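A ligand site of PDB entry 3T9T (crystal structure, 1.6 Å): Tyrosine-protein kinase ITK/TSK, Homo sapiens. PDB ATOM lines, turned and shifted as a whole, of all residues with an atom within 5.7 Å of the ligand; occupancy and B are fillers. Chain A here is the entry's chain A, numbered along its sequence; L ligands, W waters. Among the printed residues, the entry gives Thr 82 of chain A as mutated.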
ATOM      1  N   ILE A  16      15.291   2.323  15.606  1.00  0.00           N
ATOM      2  CA  ILE A  16      14.235   2.902  16.437  1.00  0.00           C
ATOM      3  C   ILE A  16      14.693   4.051  17.344  1.00  0.00           C
ATOM      4  O   ILE A  16      13.881   4.900  17.782  1.00  0.00           O
ATOM      5  CB  ILE A  16      13.406   1.827  17.192  1.00  0.00           C
ATOM      6  CG1 ILE A  16      14.248   1.070  18.233  1.00  0.00           C
ATOM      7  CG2 ILE A  16      12.733   0.872  16.191  1.00  0.00           C
ATOM      8  CD1 ILE A  16      13.423   0.104  19.122  1.00  0.00           C
ATOM      9  N   GLY A  17      15.983   4.081  17.651  1.00  0.00           N
ATOM     10  CA  GLY A  17      16.496   5.219  18.422  1.00  0.00           C
ATOM     11  C   GLY A  17      17.828   4.924  19.072  1.00  0.00           C
ATOM     12  O   GLY A  17      18.449   3.924  18.748  1.00  0.00           O
ATOM     13  N   SER A  18      18.249   5.804  19.972  1.00  0.00           N
ATOM     14  CA  SER A  18      19.560   5.704  20.656  1.00  0.00           C
ATOM     15  C   SER A  18      19.356   5.575  22.160  1.00  0.00           C
ATOM     16  O   SER A  18      18.584   6.332  22.763  1.00  0.00           O
ATOM     17  CB  SER A  18      20.398   6.952  20.382  1.00  0.00           C
ATOM     18  OG  SER A  18      21.043   6.843  19.124  1.00  0.00           O
ATOM     19  N   GLY A  19      20.063   4.623  22.751  1.00  0.00           N
ATOM     20  CA  GLY A  19      20.034   4.398  24.189  1.00  0.00           C
ATOM     21  C   GLY A  19      21.456   4.373  24.733  1.00  0.00           C
ATOM     22  O   GLY A  19      22.431   4.757  24.058  1.00  0.00           O
ATOM     23  N   VAL A  24      19.685   1.508  18.573  1.00  0.00           N
ATOM     24  CA  VAL A  24      18.828   0.327  18.735  1.00  0.00           C
ATOM     25  C   VAL A  24      17.943   0.139  17.502  1.00  0.00           C
ATOM     26  O   VAL A  24      17.415   1.106  16.955  1.00  0.00           O
ATOM     27  CB  VAL A  24      18.020   0.390  20.061  1.00  0.00           C
ATOM     28  CG1 VAL A  24      17.149  -0.844  20.257  1.00  0.00           C
ATOM     29  CG2 VAL A  24      18.977   0.566  21.254  1.00  0.00           C
ATOM     30  N   ALA A  36      14.658  -6.386  19.941  1.00  0.00           N
ATOM     31  CA  ALA A  36      15.444  -5.163  19.827  1.00  0.00           C
ATOM     32  C   ALA A  36      16.911  -5.524  19.810  1.00  0.00           C
ATOM     33  O   ALA A  36      17.342  -6.462  20.496  1.00  0.00           O
ATOM     34  CB  ALA A  36      15.153  -4.195  21.016  1.00  0.00           C
ATOM     35  N   ILE A  37      17.684  -4.802  19.015  1.00  0.00           N
ATOM     36  CA  ILE A  37      19.116  -5.089  18.922  1.00  0.00           C
ATOM     37  C   ILE A  37      19.862  -3.808  19.120  1.00  0.00           C
ATOM     38  O   ILE A  37      19.633  -2.836  18.378  1.00  0.00           O
ATOM     39  CB  ILE A  37      19.511  -5.653  17.530  1.00  0.00           C
ATOM     40  CG1 ILE A  37      18.625  -6.843  17.135  1.00  0.00           C
ATOM     41  CG2 ILE A  37      20.975  -6.086  17.518  1.00  0.00           C
ATOM     42  CD1 ILE A  37      18.800  -7.241  15.682  1.00  0.00           C
ATOM     43  N   LYS A  38      20.760  -3.776  20.116  1.00  0.00           N
ATOM     44  CA  LYS A  38      21.536  -2.556  20.350  1.00  0.00           C
ATOM     45  C   LYS A  38      22.935  -2.803  19.838  1.00  0.00           C
ATOM     46  O   LYS A  38      23.593  -3.790  20.222  1.00  0.00           O
ATOM     47  CB  LYS A  38      21.578  -2.209  21.850  1.00  0.00           C
ATOM     48  CG  LYS A  38      22.357  -0.937  22.155  1.00  0.00           C
ATOM     49  CD  LYS A  38      22.443  -0.729  23.660  1.00  0.00           C
ATOM     50  CE  LYS A  38      21.142  -0.222  24.222  1.00  0.00           C
ATOM     51  NZ  LYS A  38      21.309   0.137  25.686  1.00  0.00           N
ATOM     52  N   VAL A  66      13.400  -5.900  31.505  1.00  0.00           N
ATOM     53  CA  VAL A  66      13.765  -6.168  30.116  1.00  0.00           C
ATOM     54  C   VAL A  66      14.696  -7.358  29.989  1.00  0.00           C
ATOM     55  O   VAL A  66      15.772  -7.381  30.587  1.00  0.00           O
ATOM     56  CB  VAL A  66      14.439  -4.959  29.455  1.00  0.00           C
ATOM     57  CG1 VAL A  66      14.826  -5.312  28.025  1.00  0.00           C
ATOM     58  CG2 VAL A  66      13.472  -3.786  29.460  1.00  0.00           C
ATOM     59  N   LEU A  68      17.350  -9.788  28.614  1.00  0.00           N
ATOM     60  CA  LEU A  68      18.484 -10.025  27.716  1.00  0.00           C
ATOM     61  C   LEU A  68      18.407 -11.415  27.094  1.00  0.00           C
ATOM     62  O   LEU A  68      18.339 -12.422  27.819  1.00  0.00           O
ATOM     63  CB  LEU A  68      19.807  -9.873  28.447  1.00  0.00           C
ATOM     64  CG  LEU A  68      21.092  -9.944  27.603  1.00  0.00           C
ATOM     65  CD1 LEU A  68      21.145  -8.757  26.632  1.00  0.00           C
ATOM     66  CD2 LEU A  68      22.307  -9.869  28.535  1.00  0.00           C
ATOM     67  N   LEU A  80      23.865  -6.260  21.636  1.00  0.00           N
ATOM     68  CA  LEU A  80      23.023  -6.941  22.642  1.00  0.00           C
ATOM     69  C   LEU A  80      21.597  -7.066  22.117  1.00  0.00           C
ATOM     70  O   LEU A  80      21.066  -6.130  21.501  1.00  0.00           O
ATOM     71  CB  LEU A  80      22.989  -6.134  23.955  1.00  0.00           C
ATOM     72  CG  LEU A  80      24.194  -6.224  24.913  1.00  0.00           C
ATOM     73  CD1 LEU A  80      25.543  -6.017  24.196  1.00  0.00           C
ATOM     74  CD2 LEU A  80      24.046  -5.197  26.063  1.00  0.00           C
ATOM     75  N   VAL A  81      20.981  -8.214  22.396  1.00  0.00           N
ATOM     76  CA  VAL A  81      19.640  -8.527  21.887  1.00  0.00           C
ATOM     77  C   VAL A  81      18.680  -8.725  23.060  1.00  0.00           C
ATOM     78  O   VAL A  81      18.960  -9.489  23.992  1.00  0.00           O
ATOM     79  CB  VAL A  81      19.689  -9.814  21.033  1.00  0.00           C
ATOM     80  CG1 VAL A  81      18.341 -10.078  20.381  1.00  0.00           C
ATOM     81  CG2 VAL A  81      20.796  -9.697  19.996  1.00  0.00           C
ATOM     82  N   THR A  82      17.536  -8.054  22.994  1.00  0.00           N
ATOM     83  CA  THR A  82      16.506  -8.196  24.031  1.00  0.00           C
ATOM     84  C   THR A  82      15.102  -8.306  23.454  1.00  0.00           C
ATOM     85  O   THR A  82      14.879  -8.155  22.234  1.00  0.00           O
ATOM     86  CB  THR A  82      16.443  -6.983  24.997  1.00  0.00           C
ATOM     87  OG1 THR A  82      15.898  -5.817  24.333  1.00  0.00           O
ATOM     88  CG2 THR A  82      17.811  -6.688  25.570  1.00  0.00           C
ATOM     89  N   GLU A  83      14.162  -8.544  24.349  1.00  0.00           N
ATOM     90  CA  GLU A  83      12.767  -8.455  23.988  1.00  0.00           C
ATOM     91  C   GLU A  83      12.464  -7.078  23.456  1.00  0.00           C
ATOM     92  O   GLU A  83      13.121  -6.115  23.805  1.00  0.00           O
ATOM     93  CB  GLU A  83      11.868  -8.769  25.185  1.00  0.00           C
ATOM     94  CG  GLU A  83      11.816  -7.668  26.238  1.00  0.00           C
ATOM     95  CD  GLU A  83      10.906  -8.051  27.395  1.00  0.00           C
ATOM     96  OE1 GLU A  83      11.435  -8.333  28.492  1.00  0.00           O
ATOM     97  OE2 GLU A  83       9.674  -8.077  27.205  1.00  0.00           O
ATOM     98  N   PHE A  84      11.488  -7.000  22.554  1.00  0.00           N
ATOM     99  CA  PHE A  84      11.085  -5.716  21.969  1.00  0.00           C
ATOM    100  C   PHE A  84       9.937  -5.067  22.746  1.00  0.00           C
ATOM    101  O   PHE A  84       8.906  -5.725  23.023  1.00  0.00           O
ATOM    102  CB  PHE A  84      10.670  -5.929  20.507  1.00  0.00           C
ATOM    103  CG  PHE A  84      10.201  -4.666  19.835  1.00  0.00           C
ATOM    104  CD1 PHE A  84      11.070  -3.629  19.574  1.00  0.00           C
ATOM    105  CD2 PHE A  84       8.877  -4.530  19.473  1.00  0.00           C
ATOM    106  CE1 PHE A  84      10.630  -2.475  18.983  1.00  0.00           C
ATOM    107  CE2 PHE A  84       8.431  -3.388  18.864  1.00  0.00           C
ATOM    108  CZ  PHE A  84       9.313  -2.349  18.637  1.00  0.00           C
ATOM    109  N   MET A  85      10.107  -3.774  23.046  1.00  0.00           N
ATOM    110  CA  MET A  85       9.077  -2.979  23.739  1.00  0.00           C
ATOM    111  C   MET A  85       8.672  -1.835  22.832  1.00  0.00           C
ATOM    112  O   MET A  85       9.521  -1.092  22.361  1.00  0.00           O
ATOM    113  CB  MET A  85       9.646  -2.333  25.018  1.00  0.00           C
ATOM    114  CG  MET A  85      10.553  -3.240  25.817  1.00  0.00           C
ATOM    115  SD  MET A  85       9.542  -4.149  26.980  1.00  0.00           S
ATOM    116  CE  MET A  85       8.894  -2.828  27.987  1.00  0.00           C
ATOM    117  N   GLU A  86       7.361  -1.689  22.611  1.00  0.00           N
ATOM    118  CA  GLU A  86       6.842  -0.855  21.527  1.00  0.00           C
ATOM    119  C   GLU A  86       6.897   0.659  21.741  1.00  0.00           C
ATOM    120  O   GLU A  86       6.989   1.419  20.792  1.00  0.00           O
ATOM    121  CB  GLU A  86       5.412  -1.302  21.174  1.00  0.00           C
ATOM    122  CG  GLU A  86       5.328  -2.789  20.760  1.00  0.00           C
ATOM    123  CD  GLU A  86       5.330  -3.798  21.951  1.00  0.00           C
ATOM    124  OE1 GLU A  86       5.476  -3.377  23.133  1.00  0.00           O
ATOM    125  OE2 GLU A  86       5.164  -5.015  21.699  1.00  0.00           O
ATOM    126  N   GLY A  88       8.880   2.851  23.820  1.00  0.00           N
ATOM    127  CA  GLY A  88      10.020   3.717  24.117  1.00  0.00           C
ATOM    128  C   GLY A  88      10.286   3.914  25.610  1.00  0.00           C
ATOM    129  O   GLY A  88       9.939   3.057  26.418  1.00  0.00           O
ATOM    130  N   CYS A  89      10.932   5.023  25.932  1.00  0.00           N
ATOM    131  CA  CYS A  89      11.319   5.356  27.319  1.00  0.00           C
ATOM    132  C   CYS A  89      10.100   5.881  28.086  1.00  0.00           C
ATOM    133  O   CYS A  89       9.277   6.666  27.553  1.00  0.00           O
ATOM    134  CB  CYS A  89      12.435   6.429  27.328  1.00  0.00           C
ATOM    135  SG  CYS A  89      14.105   5.794  26.962  1.00  0.00           S
ATOM    136  N   SER A  91      10.177   8.048  30.446  1.00  0.00           N
ATOM    137  CA  SER A  91      10.310   9.501  30.522  1.00  0.00           C
ATOM    138  C   SER A  91       9.622  10.248  29.354  1.00  0.00           C
ATOM    139  O   SER A  91       8.819  11.160  29.560  1.00  0.00           O
ATOM    140  CB  SER A  91      11.779   9.916  30.617  1.00  0.00           C
ATOM    141  OG  SER A  91      12.554   9.273  29.615  1.00  0.00           O
ATOM    142  N   ASP A  92       9.968   9.859  28.137  1.00  0.00           N
ATOM    143  CA  ASP A  92       9.365  10.437  26.934  1.00  0.00           C
ATOM    144  C   ASP A  92       7.888  10.136  26.866  1.00  0.00           C
ATOM    145  O   ASP A  92       7.103  10.961  26.433  1.00  0.00           O
ATOM    146  CB  ASP A  92       9.978   9.785  25.692  1.00  0.00           C
ATOM    147  CG  ASP A  92      11.425  10.179  25.490  1.00  0.00           C
ATOM    148  OD1 ASP A  92      11.819  11.257  25.956  1.00  0.00           O
ATOM    149  OD2 ASP A  92      12.154   9.378  24.852  1.00  0.00           O
ATOM    150  N   ARG A 133      14.095   7.596  32.702  1.00  0.00           N
ATOM    151  CA  ARG A 133      14.764   7.571  31.412  1.00  0.00           C
ATOM    152  C   ARG A 133      15.287   6.204  31.021  1.00  0.00           C
ATOM    153  O   ARG A 133      15.581   5.991  29.840  1.00  0.00           O
ATOM    154  CB  ARG A 133      15.892   8.602  31.389  1.00  0.00           C
ATOM    155  CG  ARG A 133      16.970   8.281  32.418  1.00  0.00           C
ATOM    156  CD  ARG A 133      18.083   9.341  32.471  1.00  0.00           C
ATOM    157  NE  ARG A 133      18.613   9.479  33.831  1.00  0.00           N
ATOM    158  CZ  ARG A 133      19.464   8.624  34.394  1.00  0.00           C
ATOM    159  NH1 ARG A 133      19.870   8.822  35.646  1.00  0.00           N
ATOM    160  NH2 ARG A 133      19.913   7.567  33.715  1.00  0.00           N
ATOM    161  N   LEU A 136      11.357   1.195  30.157  1.00  0.00           N
ATOM    162  CA  LEU A 136      10.750   1.088  28.826  1.00  0.00           C
ATOM    163  C   LEU A 136       9.271   0.738  28.982  1.00  0.00           C
ATOM    164  O   LEU A 136       8.853   0.143  29.982  1.00  0.00           O
ATOM    165  CB  LEU A 136      11.456   0.006  27.976  1.00  0.00           C
ATOM    166  CG  LEU A 136      12.926   0.342  27.686  1.00  0.00           C
ATOM    167  CD1 LEU A 136      13.567  -0.767  26.860  1.00  0.00           C
ATOM    168  CD2 LEU A 136      13.057   1.691  27.017  1.00  0.00           C
ATOM    169  N   SER A 146      15.146  -1.407  32.811  1.00  0.00           N
ATOM    170  CA  SER A 146      16.236  -1.718  31.872  1.00  0.00           C
ATOM    171  C   SER A 146      17.563  -1.117  32.371  1.00  0.00           C
ATOM    172  O   SER A 146      17.563  -0.208  33.198  1.00  0.00           O
ATOM    173  CB  SER A 146      15.918  -1.110  30.497  1.00  0.00           C
ATOM    174  OG  SER A 146      16.831  -1.580  29.520  1.00  0.00           O
ATOM    175  N   ASP A 147      18.668  -1.603  31.809  1.00  0.00           N
ATOM    176  CA  ASP A 147      20.019  -1.045  32.014  1.00  0.00           C
ATOM    177  C   ASP A 147      20.547  -1.304  33.433  1.00  0.00           C
ATOM    178  O   ASP A 147      21.483  -0.632  33.861  1.00  0.00           O
ATOM    179  CB  ASP A 147      20.079   0.479  31.708  1.00  0.00           C
ATOM    180  CG  ASP A 147      19.835   0.829  30.233  1.00  0.00           C
ATOM    181  OD1 ASP A 147      19.819   2.065  29.901  1.00  0.00           O
ATOM    182  OD2 ASP A 147      19.625  -0.088  29.418  1.00  0.00           O
HETATM  183  C1  LIG L   1      20.118  -3.730  24.976  1.00  0.00           C
HETATM  184  C2  LIG L   1      20.363  -3.277  26.275  1.00  0.00           C
HETATM  185  C3  LIG L   1      19.345  -2.722  27.035  1.00  0.00           C
HETATM  186  C4  LIG L   1      18.559  -4.119  23.033  1.00  0.00           C
HETATM  187  C5  LIG L   1      13.973   1.518  22.680  1.00  0.00           C
HETATM  188  C6  LIG L   1      15.965   2.829  23.077  1.00  0.00           C
HETATM  189  C7  LIG L   1      12.730  -1.258  22.862  1.00  0.00           C
HETATM  190  C8  LIG L   1      13.576   3.817  20.712  1.00  0.00           C
HETATM  191  C9  LIG L   1      13.838   4.835  24.369  1.00  0.00           C
HETATM  192  C10 LIG L   1      14.682   5.624  25.044  1.00  0.00           C
HETATM  193  O1  LIG L   1      13.269   5.997  22.474  1.00  0.00           O
HETATM  194  C11 LIG L   1      13.703   4.927  22.905  1.00  0.00           C
HETATM  195  C12 LIG L   1      15.663   6.597  24.460  1.00  0.00           C
HETATM  196  N1  LIG L   1      15.966   7.712  25.350  1.00  0.00           N
HETATM  197  C13 LIG L   1      15.211   8.900  24.949  1.00  0.00           C
HETATM  198  C14 LIG L   1      17.395   7.994  25.324  1.00  0.00           C
HETATM  199  N2  LIG L   1      13.987   3.879  22.114  1.00  0.00           N
HETATM  200  C15 LIG L   1      14.645   2.745  22.632  1.00  0.00           C
HETATM  201  F1  LIG L   1      16.652   3.991  23.056  1.00  0.00           F
HETATM  202  C16 LIG L   1      16.590   1.689  23.593  1.00  0.00           C
HETATM  203  C17 LIG L   1      15.919   0.471  23.646  1.00  0.00           C
HETATM  204  N3  LIG L   1      16.581  -0.613  24.156  1.00  0.00           N
HETATM  205  C18 LIG L   1      14.601   0.367  23.175  1.00  0.00           C
HETATM  206  N4  LIG L   1      13.963  -0.892  23.249  1.00  0.00           N
HETATM  207  N5  LIG L   1      12.556  -2.578  23.110  1.00  0.00           N
HETATM  208  C19 LIG L   1      13.684  -3.068  23.672  1.00  0.00           C
HETATM  209  C20 LIG L   1      14.588  -1.955  23.752  1.00  0.00           C
HETATM  210  C21 LIG L   1      15.984  -1.822  24.233  1.00  0.00           C
HETATM  211  N6  LIG L   1      16.558  -2.950  24.704  1.00  0.00           N
HETATM  212  C22 LIG L   1      17.808  -3.053  25.210  1.00  0.00           C
HETATM  213  C23 LIG L   1      18.823  -3.625  24.440  1.00  0.00           C
HETATM  214  C24 LIG L   1      18.053  -2.600  26.509  1.00  0.00           C
HETATM  215  O   HOH W   1      18.561   0.537  25.616  1.00  0.00           O
HETATM  216  O   HOH W   2      11.060   7.174  23.847  1.00  0.00           O
HETATM  217  O   HOH W   3      10.617   1.413  21.823  1.00  0.00           O
HETATM  218  O   HOH W   4      15.834   7.550  21.070  1.00  0.00           O
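A carbon (C10) of the ligand is covalently linked to the side-chain sulfur (SG) of Cys 89 (2.0 Å). N of Met 85 is in hydrogen-bond range of N5 of the ligand. OG1 of Thr 82 sits at hydrogen-bond distance from N6 of the ligand, at 3.0 Å.
N of Ala 36 sits at hydrogen-bond distance from O of Thr 82 (2.9 Å). The backbone NH (N) of Ile 16 is in hydrogen-bond range of the backbone carbonyl oxygen (O) of Val 24, at 2.8 Å. The side-chain hydroxyl of Ser 146 lies within hydrogen-bond range of the side-chain carboxylate of Asp 147, at 3.2 Å. The backbone NH (N) of Val 24 sits at hydrogen-bond distance from the backbone carbonyl oxygen (O) of Gly 17 (2.7 Å). The backbone carbonyl oxygen (O) of Leu 80 lies within hydrogen-bond range of the backbone NH (N) of Lys 38 (2.7 Å).
O of Ser 18 lies close to F1 of the ligand (3.0 Å). The backbone NH (N) of Gly 19 lies close to a fluorine (F1) of the ligand, at 3.5 Å. Merely in contact with the ligand: Asp 92, Glu 83, Ile 16, Ala 36, Ser 146, Leu 136, Val 24, Leu 80, Asp 147, Lys 38, Phe 84, Gly 88 and Gly 17. Hydrophobic or aromatic side chains within 4 Å of the ligand: Ile 16, Val 24, Ala 36, Leu 80, Phe 84, Met 85 and Leu 136. Of the 25 residues printed, 18 come within 4 Å of the ligand. The nearest printed residue that does not touch the ligand is Ile 37 (4.1 Å).
Water W1 lies within hydrogen-bond range of a nitrogen (N3) of the ligand (2.7 Å) and the side-chain amino group (NZ) of Lys 38 (2.8 Å). Water W2 lies within hydrogen-bond range of OD2 of Asp 92 (2.7 Å), O1 of the ligand (2.9 Å) and N of Cys 89 (3.0 Å). Water W4 bridges the backbone NH of Ser 18 (3.2 Å) and an oxygen (O1) of the ligand (3.3 Å).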
